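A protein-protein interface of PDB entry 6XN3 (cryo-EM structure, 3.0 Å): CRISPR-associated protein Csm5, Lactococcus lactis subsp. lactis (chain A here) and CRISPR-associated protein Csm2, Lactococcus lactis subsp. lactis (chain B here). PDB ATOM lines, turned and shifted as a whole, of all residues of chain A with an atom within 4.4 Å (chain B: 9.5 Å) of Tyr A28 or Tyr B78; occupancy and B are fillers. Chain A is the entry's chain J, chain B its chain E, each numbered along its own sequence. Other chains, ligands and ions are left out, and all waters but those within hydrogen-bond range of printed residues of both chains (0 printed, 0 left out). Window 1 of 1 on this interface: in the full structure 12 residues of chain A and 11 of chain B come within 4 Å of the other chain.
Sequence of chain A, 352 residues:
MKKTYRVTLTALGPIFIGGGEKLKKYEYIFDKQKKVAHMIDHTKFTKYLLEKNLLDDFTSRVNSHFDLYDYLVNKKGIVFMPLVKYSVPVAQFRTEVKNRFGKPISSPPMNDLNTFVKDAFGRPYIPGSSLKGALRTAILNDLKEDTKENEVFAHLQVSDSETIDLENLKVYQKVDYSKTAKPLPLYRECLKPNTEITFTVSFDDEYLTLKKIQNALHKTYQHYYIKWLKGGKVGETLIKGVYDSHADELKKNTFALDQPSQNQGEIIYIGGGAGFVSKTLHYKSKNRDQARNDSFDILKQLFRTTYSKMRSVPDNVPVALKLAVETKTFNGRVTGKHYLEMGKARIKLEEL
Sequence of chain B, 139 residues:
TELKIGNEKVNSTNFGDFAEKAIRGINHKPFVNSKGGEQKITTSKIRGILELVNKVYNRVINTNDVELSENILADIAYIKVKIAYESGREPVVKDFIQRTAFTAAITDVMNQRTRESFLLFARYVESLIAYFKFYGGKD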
ATOM      1  N   LEU A  23      26.827 -12.853 -10.563  1.00  0.00           N
ATOM      2  CA  LEU A  23      27.040 -14.044  -9.753  1.00  0.00           C
ATOM      3  C   LEU A  23      27.281 -13.607  -8.317  1.00  0.00           C
ATOM      4  O   LEU A  23      28.203 -12.830  -8.048  1.00  0.00           O
ATOM      5  CB  LEU A  23      28.217 -14.863 -10.287  1.00  0.00           C
ATOM      6  CG  LEU A  23      28.028 -15.850 -11.447  1.00  0.00           C
ATOM      7  CD1 LEU A  23      27.119 -16.929 -11.025  1.00  0.00           C
ATOM      8  CD2 LEU A  23      27.449 -15.240 -12.701  1.00  0.00           C
ATOM      9  N   TYR A  26      27.208 -16.816  -2.767  1.00  0.00           N
ATOM     10  CA  TYR A  26      27.126 -18.226  -3.150  1.00  0.00           C
ATOM     11  C   TYR A  26      25.825 -18.418  -3.919  1.00  0.00           C
ATOM     12  O   TYR A  26      24.814 -18.862  -3.373  1.00  0.00           O
ATOM     13  CB  TYR A  26      27.206 -19.156  -1.945  1.00  0.00           C
ATOM     14  CG  TYR A  26      27.221 -20.627  -2.311  1.00  0.00           C
ATOM     15  CD1 TYR A  26      28.305 -21.191  -2.969  1.00  0.00           C
ATOM     16  CD2 TYR A  26      26.145 -21.449  -2.001  1.00  0.00           C
ATOM     17  CE1 TYR A  26      28.309 -22.528  -3.314  1.00  0.00           C
ATOM     18  CE2 TYR A  26      26.149 -22.789  -2.338  1.00  0.00           C
ATOM     19  CZ  TYR A  26      27.237 -23.320  -2.993  1.00  0.00           C
ATOM     20  OH  TYR A  26      27.256 -24.650  -3.335  1.00  0.00           O
ATOM     21  N   GLU A  27      25.866 -18.106  -5.210  1.00  0.00           N
ATOM     22  CA  GLU A  27      24.749 -18.356  -6.123  1.00  0.00           C
ATOM     23  C   GLU A  27      25.423 -18.727  -7.443  1.00  0.00           C
ATOM     24  O   GLU A  27      25.887 -17.850  -8.170  1.00  0.00           O
ATOM     25  CB  GLU A  27      23.833 -17.145  -6.283  1.00  0.00           C
ATOM     26  CG  GLU A  27      23.049 -16.707  -5.028  1.00  0.00           C
ATOM     27  CD  GLU A  27      22.011 -17.701  -4.566  1.00  0.00           C
ATOM     28  OE1 GLU A  27      21.436 -18.397  -5.416  1.00  0.00           O
ATOM     29  OE2 GLU A  27      21.796 -17.811  -3.342  1.00  0.00           O
ATOM     30  N   TYR A  28      25.531 -20.035  -7.693  1.00  0.00           N
ATOM     31  CA  TYR A  28      26.231 -20.734  -8.787  1.00  0.00           C
ATOM     32  C   TYR A  28      27.752 -20.637  -8.711  1.00  0.00           C
ATOM     33  O   TYR A  28      28.425 -21.320  -9.488  1.00  0.00           O
ATOM     34  CB  TYR A  28      25.833 -20.297 -10.209  1.00  0.00           C
ATOM     35  CG  TYR A  28      24.391 -19.931 -10.426  1.00  0.00           C
ATOM     36  CD1 TYR A  28      23.409 -20.901 -10.430  1.00  0.00           C
ATOM     37  CD2 TYR A  28      24.019 -18.619 -10.686  1.00  0.00           C
ATOM     38  CE1 TYR A  28      22.102 -20.571 -10.651  1.00  0.00           C
ATOM     39  CE2 TYR A  28      22.707 -18.278 -10.903  1.00  0.00           C
ATOM     40  CZ  TYR A  28      21.749 -19.261 -10.885  1.00  0.00           C
ATOM     41  OH  TYR A  28      20.430 -18.933 -11.103  1.00  0.00           O
ATOM     42  N   ILE A  29      28.319 -19.846  -7.818  1.00  0.00           N
ATOM     43  CA  ILE A  29      29.762 -19.674  -7.750  1.00  0.00           C
ATOM     44  C   ILE A  29      30.314 -20.719  -6.790  1.00  0.00           C
ATOM     45  O   ILE A  29      29.633 -21.138  -5.851  1.00  0.00           O
ATOM     46  CB  ILE A  29      30.120 -18.236  -7.324  1.00  0.00           C
ATOM     47  CG1 ILE A  29      31.616 -17.941  -7.448  1.00  0.00           C
ATOM     48  CG2 ILE A  29      29.612 -17.921  -5.949  1.00  0.00           C
ATOM     49  CD1 ILE A  29      31.937 -16.475  -7.331  1.00  0.00           C
ATOM     50  N   PHE A  30      31.510 -21.216  -7.080  1.00  0.00           N
ATOM     51  CA  PHE A  30      32.164 -22.238  -6.274  1.00  0.00           C
ATOM     52  C   PHE A  30      33.632 -21.844  -6.176  1.00  0.00           C
ATOM     53  O   PHE A  30      34.441 -22.184  -7.041  1.00  0.00           O
ATOM     54  CB  PHE A  30      31.957 -23.603  -6.913  1.00  0.00           C
ATOM     55  CG  PHE A  30      32.552 -24.736  -6.154  1.00  0.00           C
ATOM     56  CD1 PHE A  30      31.948 -25.217  -5.012  1.00  0.00           C
ATOM     57  CD2 PHE A  30      33.716 -25.337  -6.596  1.00  0.00           C
ATOM     58  CE1 PHE A  30      32.501 -26.278  -4.313  1.00  0.00           C
ATOM     59  CE2 PHE A  30      34.272 -26.396  -5.908  1.00  0.00           C
ATOM     60  CZ  PHE A  30      33.667 -26.863  -4.763  1.00  0.00           C
ATOM     61  N   MET A  39      32.533 -22.942 -11.618  1.00  0.00           N
ATOM     62  CA  MET A  39      31.145 -22.519 -11.621  1.00  0.00           C
ATOM     63  C   MET A  39      30.259 -23.572 -12.259  1.00  0.00           C
ATOM     64  O   MET A  39      30.694 -24.363 -13.101  1.00  0.00           O
ATOM     65  CB  MET A  39      30.960 -21.178 -12.306  1.00  0.00           C
ATOM     66  CG  MET A  39      31.285 -21.138 -13.759  1.00  0.00           C
ATOM     67  SD  MET A  39      31.066 -19.425 -14.223  1.00  0.00           S
ATOM     68  CE  MET A  39      32.515 -18.762 -13.423  1.00  0.00           C
ATOM     69  N   ILE A  40      29.002 -23.561 -11.831  1.00  0.00           N
ATOM     70  CA  ILE A  40      28.083 -24.668 -12.006  1.00  0.00           C
ATOM     71  C   ILE A  40      26.955 -24.234 -12.928  1.00  0.00           C
ATOM     72  O   ILE A  40      26.805 -23.056 -13.255  1.00  0.00           O
ATOM     73  CB  ILE A  40      27.536 -25.153 -10.654  1.00  0.00           C
ATOM     74  CG1 ILE A  40      26.492 -24.169 -10.139  1.00  0.00           C
ATOM     75  CG2 ILE A  40      28.662 -25.291  -9.641  1.00  0.00           C
ATOM     76  CD1 ILE A  40      26.011 -24.458  -8.747  1.00  0.00           C
ATOM     77  N   HIS A  42      22.754 -24.213 -13.448  1.00  0.00           N
ATOM     78  CA  HIS A  42      21.589 -24.131 -12.572  1.00  0.00           C
ATOM     79  C   HIS A  42      20.711 -25.377 -12.646  1.00  0.00           C
ATOM     80  O   HIS A  42      20.179 -25.821 -11.620  1.00  0.00           O
ATOM     81  CB  HIS A  42      20.789 -22.877 -12.909  1.00  0.00           C
ATOM     82  CG  HIS A  42      20.203 -22.875 -14.282  1.00  0.00           C
ATOM     83  ND1 HIS A  42      20.933 -22.542 -15.403  1.00  0.00           N
ATOM     84  CD2 HIS A  42      18.963 -23.184 -14.721  1.00  0.00           C
ATOM     85  CE1 HIS A  42      20.160 -22.631 -16.472  1.00  0.00           C
ATOM     86  NE2 HIS A  42      18.958 -23.016 -16.084  1.00  0.00           N
ATOM     87  N   PHE A  45      22.502 -28.445 -10.976  1.00  0.00           N
ATOM     88  CA  PHE A  45      22.567 -28.174  -9.540  1.00  0.00           C
ATOM     89  C   PHE A  45      21.218 -28.401  -8.883  1.00  0.00           C
ATOM     90  O   PHE A  45      21.122 -29.089  -7.862  1.00  0.00           O
ATOM     91  CB  PHE A  45      23.033 -26.741  -9.283  1.00  0.00           C
ATOM     92  CG  PHE A  45      23.305 -26.423  -7.829  1.00  0.00           C
ATOM     93  CD1 PHE A  45      24.123 -27.234  -7.064  1.00  0.00           C
ATOM     94  CD2 PHE A  45      22.765 -25.292  -7.243  1.00  0.00           C
ATOM     95  CE1 PHE A  45      24.396 -26.931  -5.743  1.00  0.00           C
ATOM     96  CE2 PHE A  45      23.034 -24.981  -5.918  1.00  0.00           C
ATOM     97  CZ  PHE A  45      23.856 -25.799  -5.172  1.00  0.00           C
ATOM     98  N   THR A  46      20.158 -27.843  -9.473  1.00  0.00           N
ATOM     99  CA  THR A  46      18.851 -27.930  -8.840  1.00  0.00           C
ATOM    100  C   THR A  46      18.314 -29.355  -8.858  1.00  0.00           C
ATOM    101  O   THR A  46      17.772 -29.808  -7.851  1.00  0.00           O
ATOM    102  CB  THR A  46      17.878 -26.962  -9.506  1.00  0.00           C
ATOM    103  OG1 THR A  46      18.449 -25.649  -9.494  1.00  0.00           O
ATOM    104  CG2 THR A  46      16.573 -26.904  -8.726  1.00  0.00           C
ATOM    105  N   LEU B  52      15.716 -11.365 -12.909  1.00  0.00           N
ATOM    106  CA  LEU B  52      15.764 -12.817 -12.742  1.00  0.00           C
ATOM    107  C   LEU B  52      14.475 -13.488 -13.224  1.00  0.00           C
ATOM    108  O   LEU B  52      14.522 -14.508 -13.938  1.00  0.00           O
ATOM    109  CB  LEU B  52      16.115 -13.156 -11.287  1.00  0.00           C
ATOM    110  CG  LEU B  52      15.286 -12.753 -10.059  1.00  0.00           C
ATOM    111  CD1 LEU B  52      14.124 -13.654  -9.732  1.00  0.00           C
ATOM    112  CD2 LEU B  52      16.205 -12.613  -8.846  1.00  0.00           C
ATOM    113  N   VAL B  53      13.316 -12.888 -12.921  1.00  0.00           N
ATOM    114  CA  VAL B  53      12.075 -13.526 -13.355  1.00  0.00           C
ATOM    115  C   VAL B  53      11.892 -13.410 -14.869  1.00  0.00           C
ATOM    116  O   VAL B  53      11.377 -14.334 -15.507  1.00  0.00           O
ATOM    117  CB  VAL B  53      10.865 -12.985 -12.559  1.00  0.00           C
ATOM    118  CG1 VAL B  53      10.540 -11.560 -12.907  1.00  0.00           C
ATOM    119  CG2 VAL B  53       9.656 -13.859 -12.774  1.00  0.00           C
ATOM    120  N   LYS B  55      14.442 -13.287 -17.025  1.00  0.00           N
ATOM    121  CA  LYS B  55      15.408 -14.235 -17.568  1.00  0.00           C
ATOM    122  C   LYS B  55      14.817 -15.635 -17.627  1.00  0.00           C
ATOM    123  O   LYS B  55      15.078 -16.388 -18.574  1.00  0.00           O
ATOM    124  CB  LYS B  55      16.681 -14.221 -16.727  1.00  0.00           C
ATOM    125  CG  LYS B  55      17.797 -15.079 -17.285  1.00  0.00           C
ATOM    126  CD  LYS B  55      19.003 -15.073 -16.371  1.00  0.00           C
ATOM    127  CE  LYS B  55      19.734 -13.752 -16.453  1.00  0.00           C
ATOM    128  NZ  LYS B  55      20.980 -13.775 -15.652  1.00  0.00           N
ATOM    129  N   VAL B  56      14.013 -16.003 -16.627  1.00  0.00           N
ATOM    130  CA  VAL B  56      13.274 -17.262 -16.730  1.00  0.00           C
ATOM    131  C   VAL B  56      12.187 -17.161 -17.804  1.00  0.00           C
ATOM    132  O   VAL B  56      11.962 -18.106 -18.575  1.00  0.00           O
ATOM    133  CB  VAL B  56      12.696 -17.640 -15.353  1.00  0.00           C
ATOM    134  CG1 VAL B  56      11.841 -18.890 -15.435  1.00  0.00           C
ATOM    135  CG2 VAL B  56      13.813 -17.814 -14.346  1.00  0.00           C
ATOM    136  N   GLU B  70      10.992 -30.018 -16.708  1.00  0.00           N
ATOM    137  CA  GLU B  70      11.647 -30.157 -15.413  1.00  0.00           C
ATOM    138  C   GLU B  70      12.564 -28.967 -15.134  1.00  0.00           C
ATOM    139  O   GLU B  70      12.634 -28.475 -13.996  1.00  0.00           O
ATOM    140  CB  GLU B  70      12.421 -31.477 -15.376  1.00  0.00           C
ATOM    141  CG  GLU B  70      11.580 -32.775 -15.314  1.00  0.00           C
ATOM    142  CD  GLU B  70      11.003 -33.239 -16.659  1.00  0.00           C
ATOM    143  OE1 GLU B  70      10.858 -34.468 -16.843  1.00  0.00           O
ATOM    144  OE2 GLU B  70      10.678 -32.399 -17.524  1.00  0.00           O
ATOM    145  N   ASN B  71      13.245 -28.475 -16.175  1.00  0.00           N
ATOM    146  CA  ASN B  71      14.207 -27.386 -16.015  1.00  0.00           C
ATOM    147  C   ASN B  71      13.514 -26.086 -15.641  1.00  0.00           C
ATOM    148  O   ASN B  71      14.078 -25.248 -14.930  1.00  0.00           O
ATOM    149  CB  ASN B  71      14.996 -27.200 -17.308  1.00  0.00           C
ATOM    150  CG  ASN B  71      15.371 -28.511 -17.951  1.00  0.00           C
ATOM    151  OD1 ASN B  71      14.892 -28.835 -19.034  1.00  0.00           O
ATOM    152  ND2 ASN B  71      16.234 -29.271 -17.293  1.00  0.00           N
ATOM    153  N   ILE B  72      12.282 -25.903 -16.106  1.00  0.00           N
ATOM    154  CA  ILE B  72      11.545 -24.693 -15.775  1.00  0.00           C
ATOM    155  C   ILE B  72      11.144 -24.693 -14.304  1.00  0.00           C
ATOM    156  O   ILE B  72      11.270 -23.672 -13.620  1.00  0.00           O
ATOM    157  CB  ILE B  72      10.337 -24.544 -16.716  1.00  0.00           C
ATOM    158  CG1 ILE B  72      10.806 -24.479 -18.170  1.00  0.00           C
ATOM    159  CG2 ILE B  72       9.567 -23.309 -16.398  1.00  0.00           C
ATOM    160  CD1 ILE B  72      11.705 -23.317 -18.470  1.00  0.00           C
ATOM    161  N   LEU B  73      10.686 -25.838 -13.786  1.00  0.00           N
ATOM    162  CA  LEU B  73      10.404 -25.948 -12.354  1.00  0.00           C
ATOM    163  C   LEU B  73      11.666 -25.758 -11.525  1.00  0.00           C
ATOM    164  O   LEU B  73      11.614 -25.171 -10.435  1.00  0.00           O
ATOM    165  CB  LEU B  73       9.754 -27.292 -12.018  1.00  0.00           C
ATOM    166  CG  LEU B  73       8.248 -27.563 -12.161  1.00  0.00           C
ATOM    167  CD1 LEU B  73       7.445 -26.695 -11.220  1.00  0.00           C
ATOM    168  CD2 LEU B  73       7.728 -27.394 -13.555  1.00  0.00           C
ATOM    169  N   ALA B  74      12.812 -26.204 -12.050  1.00  0.00           N
ATOM    170  CA  ALA B  74      14.093 -25.868 -11.431  1.00  0.00           C
ATOM    171  C   ALA B  74      14.330 -24.362 -11.416  1.00  0.00           C
ATOM    172  O   ALA B  74      14.850 -23.822 -10.435  1.00  0.00           O
ATOM    173  CB  ALA B  74      15.230 -26.573 -12.164  1.00  0.00           C
ATOM    174  N   ASP B  75      13.934 -23.669 -12.488  1.00  0.00           N
ATOM    175  CA  ASP B  75      14.157 -22.224 -12.572  1.00  0.00           C
ATOM    176  C   ASP B  75      13.310 -21.450 -11.569  1.00  0.00           C
ATOM    177  O   ASP B  75      13.822 -20.562 -10.877  1.00  0.00           O
ATOM    178  CB  ASP B  75      13.877 -21.729 -13.988  1.00  0.00           C
ATOM    179  CG  ASP B  75      14.901 -22.210 -14.980  1.00  0.00           C
ATOM    180  OD1 ASP B  75      16.047 -22.423 -14.565  1.00  0.00           O
ATOM    181  OD2 ASP B  75      14.565 -22.359 -16.174  1.00  0.00           O
ATOM    182  N   ILE B  76      12.012 -21.760 -11.482  1.00  0.00           N
ATOM    183  CA  ILE B  76      11.178 -21.088 -10.479  1.00  0.00           C
ATOM    184  C   ILE B  76      11.597 -21.476  -9.053  1.00  0.00           C
ATOM    185  O   ILE B  76      11.607 -20.624  -8.150  1.00  0.00           O
ATOM    186  CB  ILE B  76       9.657 -21.259 -10.734  1.00  0.00           C
ATOM    187  CG1 ILE B  76       9.176 -20.601 -12.040  1.00  0.00           C
ATOM    188  CG2 ILE B  76       8.827 -20.564  -9.695  1.00  0.00           C
ATOM    189  CD1 ILE B  76       9.183 -21.351 -13.281  1.00  0.00           C
ATOM    190  N   ALA B  77      12.036 -22.724  -8.836  1.00  0.00           N
ATOM    191  CA  ALA B  77      12.556 -23.097  -7.518  1.00  0.00           C
ATOM    192  C   ALA B  77      13.825 -22.323  -7.159  1.00  0.00           C
ATOM    193  O   ALA B  77      14.004 -21.888  -6.007  1.00  0.00           O
ATOM    194  CB  ALA B  77      12.827 -24.598  -7.475  1.00  0.00           C
ATOM    195  N   TYR B  78      14.701 -22.099  -8.136  1.00  0.00           N
ATOM    196  CA  TYR B  78      15.954 -21.450  -7.790  1.00  0.00           C
ATOM    197  C   TYR B  78      15.755 -19.947  -7.652  1.00  0.00           C
ATOM    198  O   TYR B  78      16.472 -19.287  -6.895  1.00  0.00           O
ATOM    199  CB  TYR B  78      17.036 -21.746  -8.820  1.00  0.00           C
ATOM    200  CG  TYR B  78      18.390 -21.413  -8.266  1.00  0.00           C
ATOM    201  CD1 TYR B  78      19.016 -22.307  -7.408  1.00  0.00           C
ATOM    202  CD2 TYR B  78      19.006 -20.197  -8.512  1.00  0.00           C
ATOM    203  CE1 TYR B  78      20.233 -22.033  -6.860  1.00  0.00           C
ATOM    204  CE2 TYR B  78      20.212 -19.901  -7.940  1.00  0.00           C
ATOM    205  CZ  TYR B  78      20.832 -20.835  -7.136  1.00  0.00           C
ATOM    206  OH  TYR B  78      22.052 -20.550  -6.575  1.00  0.00           O
ATOM    207  N   ILE B  79      14.778 -19.375  -8.359  1.00  0.00           N
ATOM    208  CA  ILE B  79      14.554 -17.956  -8.116  1.00  0.00           C
ATOM    209  C   ILE B  79      13.806 -17.769  -6.807  1.00  0.00           C
ATOM    210  O   ILE B  79      13.916 -16.712  -6.176  1.00  0.00           O
ATOM    211  CB  ILE B  79      13.839 -17.262  -9.289  1.00  0.00           C
ATOM    212  CG1 ILE B  79      12.452 -17.830  -9.527  1.00  0.00           C
ATOM    213  CG2 ILE B  79      14.686 -17.343 -10.556  1.00  0.00           C
ATOM    214  CD1 ILE B  79      11.630 -17.039 -10.501  1.00  0.00           C
ATOM    215  N   LYS B  80      13.083 -18.798  -6.350  1.00  0.00           N
ATOM    216  CA  LYS B  80      12.553 -18.780  -4.991  1.00  0.00           C
ATOM    217  C   LYS B  80      13.673 -18.742  -3.955  1.00  0.00           C
ATOM    218  O   LYS B  80      13.614 -17.960  -2.998  1.00  0.00           O
ATOM    219  CB  LYS B  80      11.650 -19.989  -4.757  1.00  0.00           C
ATOM    220  CG  LYS B  80      11.065 -20.040  -3.371  1.00  0.00           C
ATOM    221  CD  LYS B  80      10.093 -18.908  -3.164  1.00  0.00           C
ATOM    222  CE  LYS B  80       9.383 -19.034  -1.835  1.00  0.00           C
ATOM    223  NZ  LYS B  80      10.320 -18.866  -0.694  1.00  0.00           N
ATOM    224  N   VAL B  81      14.719 -19.557  -4.139  1.00  0.00           N
ATOM    225  CA  VAL B  81      15.776 -19.502  -3.122  1.00  0.00           C
ATOM    226  C   VAL B  81      16.620 -18.235  -3.282  1.00  0.00           C
ATOM    227  O   VAL B  81      17.180 -17.731  -2.298  1.00  0.00           O
ATOM    228  CB  VAL B  81      16.655 -20.773  -3.102  1.00  0.00           C
ATOM    229  CG1 VAL B  81      15.817 -22.000  -2.768  1.00  0.00           C
ATOM    230  CG2 VAL B  81      17.464 -20.960  -4.360  1.00  0.00           C
ATOM    231  N   LYS B  82      16.673 -17.661  -4.490  1.00  0.00           N
ATOM    232  CA  LYS B  82      17.371 -16.391  -4.687  1.00  0.00           C
ATOM    233  C   LYS B  82      16.653 -15.237  -3.993  1.00  0.00           C
ATOM    234  O   LYS B  82      17.288 -14.401  -3.341  1.00  0.00           O
ATOM    235  CB  LYS B  82      17.529 -16.098  -6.180  1.00  0.00           C
ATOM    236  CG  LYS B  82      18.759 -16.711  -6.824  1.00  0.00           C
ATOM    237  CD  LYS B  82      18.784 -16.440  -8.321  1.00  0.00           C
ATOM    238  CE  LYS B  82      19.118 -14.987  -8.633  1.00  0.00           C
ATOM    239  NZ  LYS B  82      20.539 -14.635  -8.362  1.00  0.00           N
ATOM    240  N   ILE B  83      15.323 -15.174  -4.116  1.00  0.00           N
ATOM    241  CA  ILE B  83      14.613 -14.102  -3.425  1.00  0.00           C
ATOM    242  C   ILE B  83      14.539 -14.389  -1.935  1.00  0.00           C
ATOM    243  O   ILE B  83      14.387 -13.462  -1.136  1.00  0.00           O
ATOM    244  CB  ILE B  83      13.210 -13.857  -4.012  1.00  0.00           C
ATOM    245  CG1 ILE B  83      12.326 -15.089  -3.863  1.00  0.00           C
ATOM    246  CG2 ILE B  83      13.303 -13.418  -5.460  1.00  0.00           C
ATOM    247  CD1 ILE B  83      10.894 -14.846  -4.202  1.00  0.00           C
ATOM    248  N   ALA B  84      14.667 -15.658  -1.532  1.00  0.00           N
ATOM    249  CA  ALA B  84      14.842 -15.969  -0.117  1.00  0.00           C
ATOM    250  C   ALA B  84      16.144 -15.385   0.414  1.00  0.00           C
ATOM    251  O   ALA B  84      16.171 -14.791   1.500  1.00  0.00           O
ATOM    252  CB  ALA B  84      14.802 -17.481   0.094  1.00  0.00           C
ATOM    253  N   TYR B  85      17.223 -15.519  -0.361  1.00  0.00           N
ATOM    254  CA  TYR B  85      18.511 -14.929   0.003  1.00  0.00           C
ATOM    255  C   TYR B  85      18.429 -13.406   0.058  1.00  0.00           C
ATOM    256  O   TYR B  85      18.921 -12.771   1.002  1.00  0.00           O
ATOM    257  CB  TYR B  85      19.565 -15.369  -1.014  1.00  0.00           C
ATOM    258  CG  TYR B  85      20.963 -14.876  -0.744  1.00  0.00           C
ATOM    259  CD1 TYR B  85      21.737 -15.457   0.243  1.00  0.00           C
ATOM    260  CD2 TYR B  85      21.504 -13.829  -1.472  1.00  0.00           C
ATOM    261  CE1 TYR B  85      23.014 -15.021   0.497  1.00  0.00           C
ATOM    262  CE2 TYR B  85      22.782 -13.378  -1.223  1.00  0.00           C
ATOM    263  CZ  TYR B  85      23.534 -13.981  -0.235  1.00  0.00           C
ATOM    264  OH  TYR B  85      24.813 -13.542   0.023  1.00  0.00           O
ATOM    265  N   GLU B  86      17.781 -12.806  -0.942  1.00  0.00           N
ATOM    266  CA  GLU B  86      17.720 -11.350  -1.026  1.00  0.00           C
ATOM    267  C   GLU B  86      16.823 -10.764   0.055  1.00  0.00           C
ATOM    268  O   GLU B  86      17.117  -9.690   0.595  1.00  0.00           O
ATOM    269  CB  GLU B  86      17.242 -10.924  -2.412  1.00  0.00           C
ATOM    270  CG  GLU B  86      17.338  -9.438  -2.664  1.00  0.00           C
ATOM    271  CD  GLU B  86      18.763  -8.954  -2.744  1.00  0.00           C
ATOM    272  OE1 GLU B  86      19.645  -9.735  -3.158  1.00  0.00           O
ATOM    273  OE2 GLU B  86      19.005  -7.788  -2.383  1.00  0.00           O
ATOM    274  N   ILE B 106       4.678 -17.945  -6.165  1.00  0.00           N
ATOM    275  CA  ILE B 106       5.668 -18.966  -6.521  1.00  0.00           C
ATOM    276  C   ILE B 106       5.219 -20.355  -6.072  1.00  0.00           C
ATOM    277  O   ILE B 106       5.338 -21.334  -6.822  1.00  0.00           O
ATOM    278  CB  ILE B 106       7.041 -18.592  -5.934  1.00  0.00           C
ATOM    279  CG1 ILE B 106       7.529 -17.291  -6.556  1.00  0.00           C
ATOM    280  CG2 ILE B 106       8.064 -19.698  -6.157  1.00  0.00           C
ATOM    281  CD1 ILE B 106       7.743 -17.405  -8.034  1.00  0.00           C
ATOM    282  N   MET B 110       4.309 -23.718  -8.167  1.00  0.00           N
ATOM    283  CA  MET B 110       4.684 -25.084  -7.786  1.00  0.00           C
ATOM    284  C   MET B 110       3.488 -26.029  -7.768  1.00  0.00           C
ATOM    285  O   MET B 110       3.562 -27.146  -8.290  1.00  0.00           O
ATOM    286  CB  MET B 110       5.366 -25.092  -6.415  1.00  0.00           C
ATOM    287  CG  MET B 110       6.715 -24.402  -6.316  1.00  0.00           C
ATOM    288  SD  MET B 110       7.970 -25.167  -7.365  1.00  0.00           S
ATOM    289  CE  MET B 110       8.056 -24.030  -8.740  1.00  0.00           C
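OE1 of Glu A27 lies within hydrogen-bond range of OH of Tyr B78. The side-chain carboxylate (OD1) of Asp B75 sits close to a ring nitrogen (NE2) of His A42, 3.3 Å away.
O of Tyr A28 sits at hydrogen-bond distance from N of Ile A40, at 3.3 Å. OG1 of Thr A46 lies within hydrogen-bond range of O of His A42, 2.7 Å away.
Among the printed residues, merely in contact across the chains: Tyr A28 with Tyr B78 (3.2 Å), Glu A27 with Lys B82 (3.5 Å), Thr A46 with Ala B74 (3.7 Å) and Thr A46 with Tyr B78 (3.98 Å).
Tyr A28 touches just one residue of chain B: Tyr B78 (3.2 Å). Printed residues of chain A within 4 Å of Tyr B78: Glu A27, Tyr A28 and Thr A46. No residue of chain B comes within 4 Å of Ile A40. Printed residues of chain B within 4 Å of Glu A27: Tyr B78 (2.5 Å) and Lys B82 (3.5 Å). Of the printed residues of chain A, Asp B75 touches His A42 (3.0 Å). Of the printed residues of chain A, Ala B74 touches Thr A46 (3.7 Å). Of the printed residues of chain A, Lys B82 touches Glu A27. Lys B55 touches none of the printed residues of chain A. Ile A29 touches none of the printed residues of chain B. The nearest printed residue of chain A that does not touch Tyr B78 is Phe A45 (4.1 Å).
Of the 11 printed residues of chain A, 4 touch a printed residue of chain B. Hydrophobic or aromatic side chains of chain A that line the printed part of chain B: Tyr A28 and His A42. Hydrophobic or aromatic side chains of chain B within 4 Å of the printed part of chain A: Ala B74 and Tyr B78. Among the printed residues, 6 pairs touch across the chains. Among the printed residues, no Asp or Glu carboxylate lies within 4 Å of a Lys or Arg side-chain nitrogen of the other chain.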
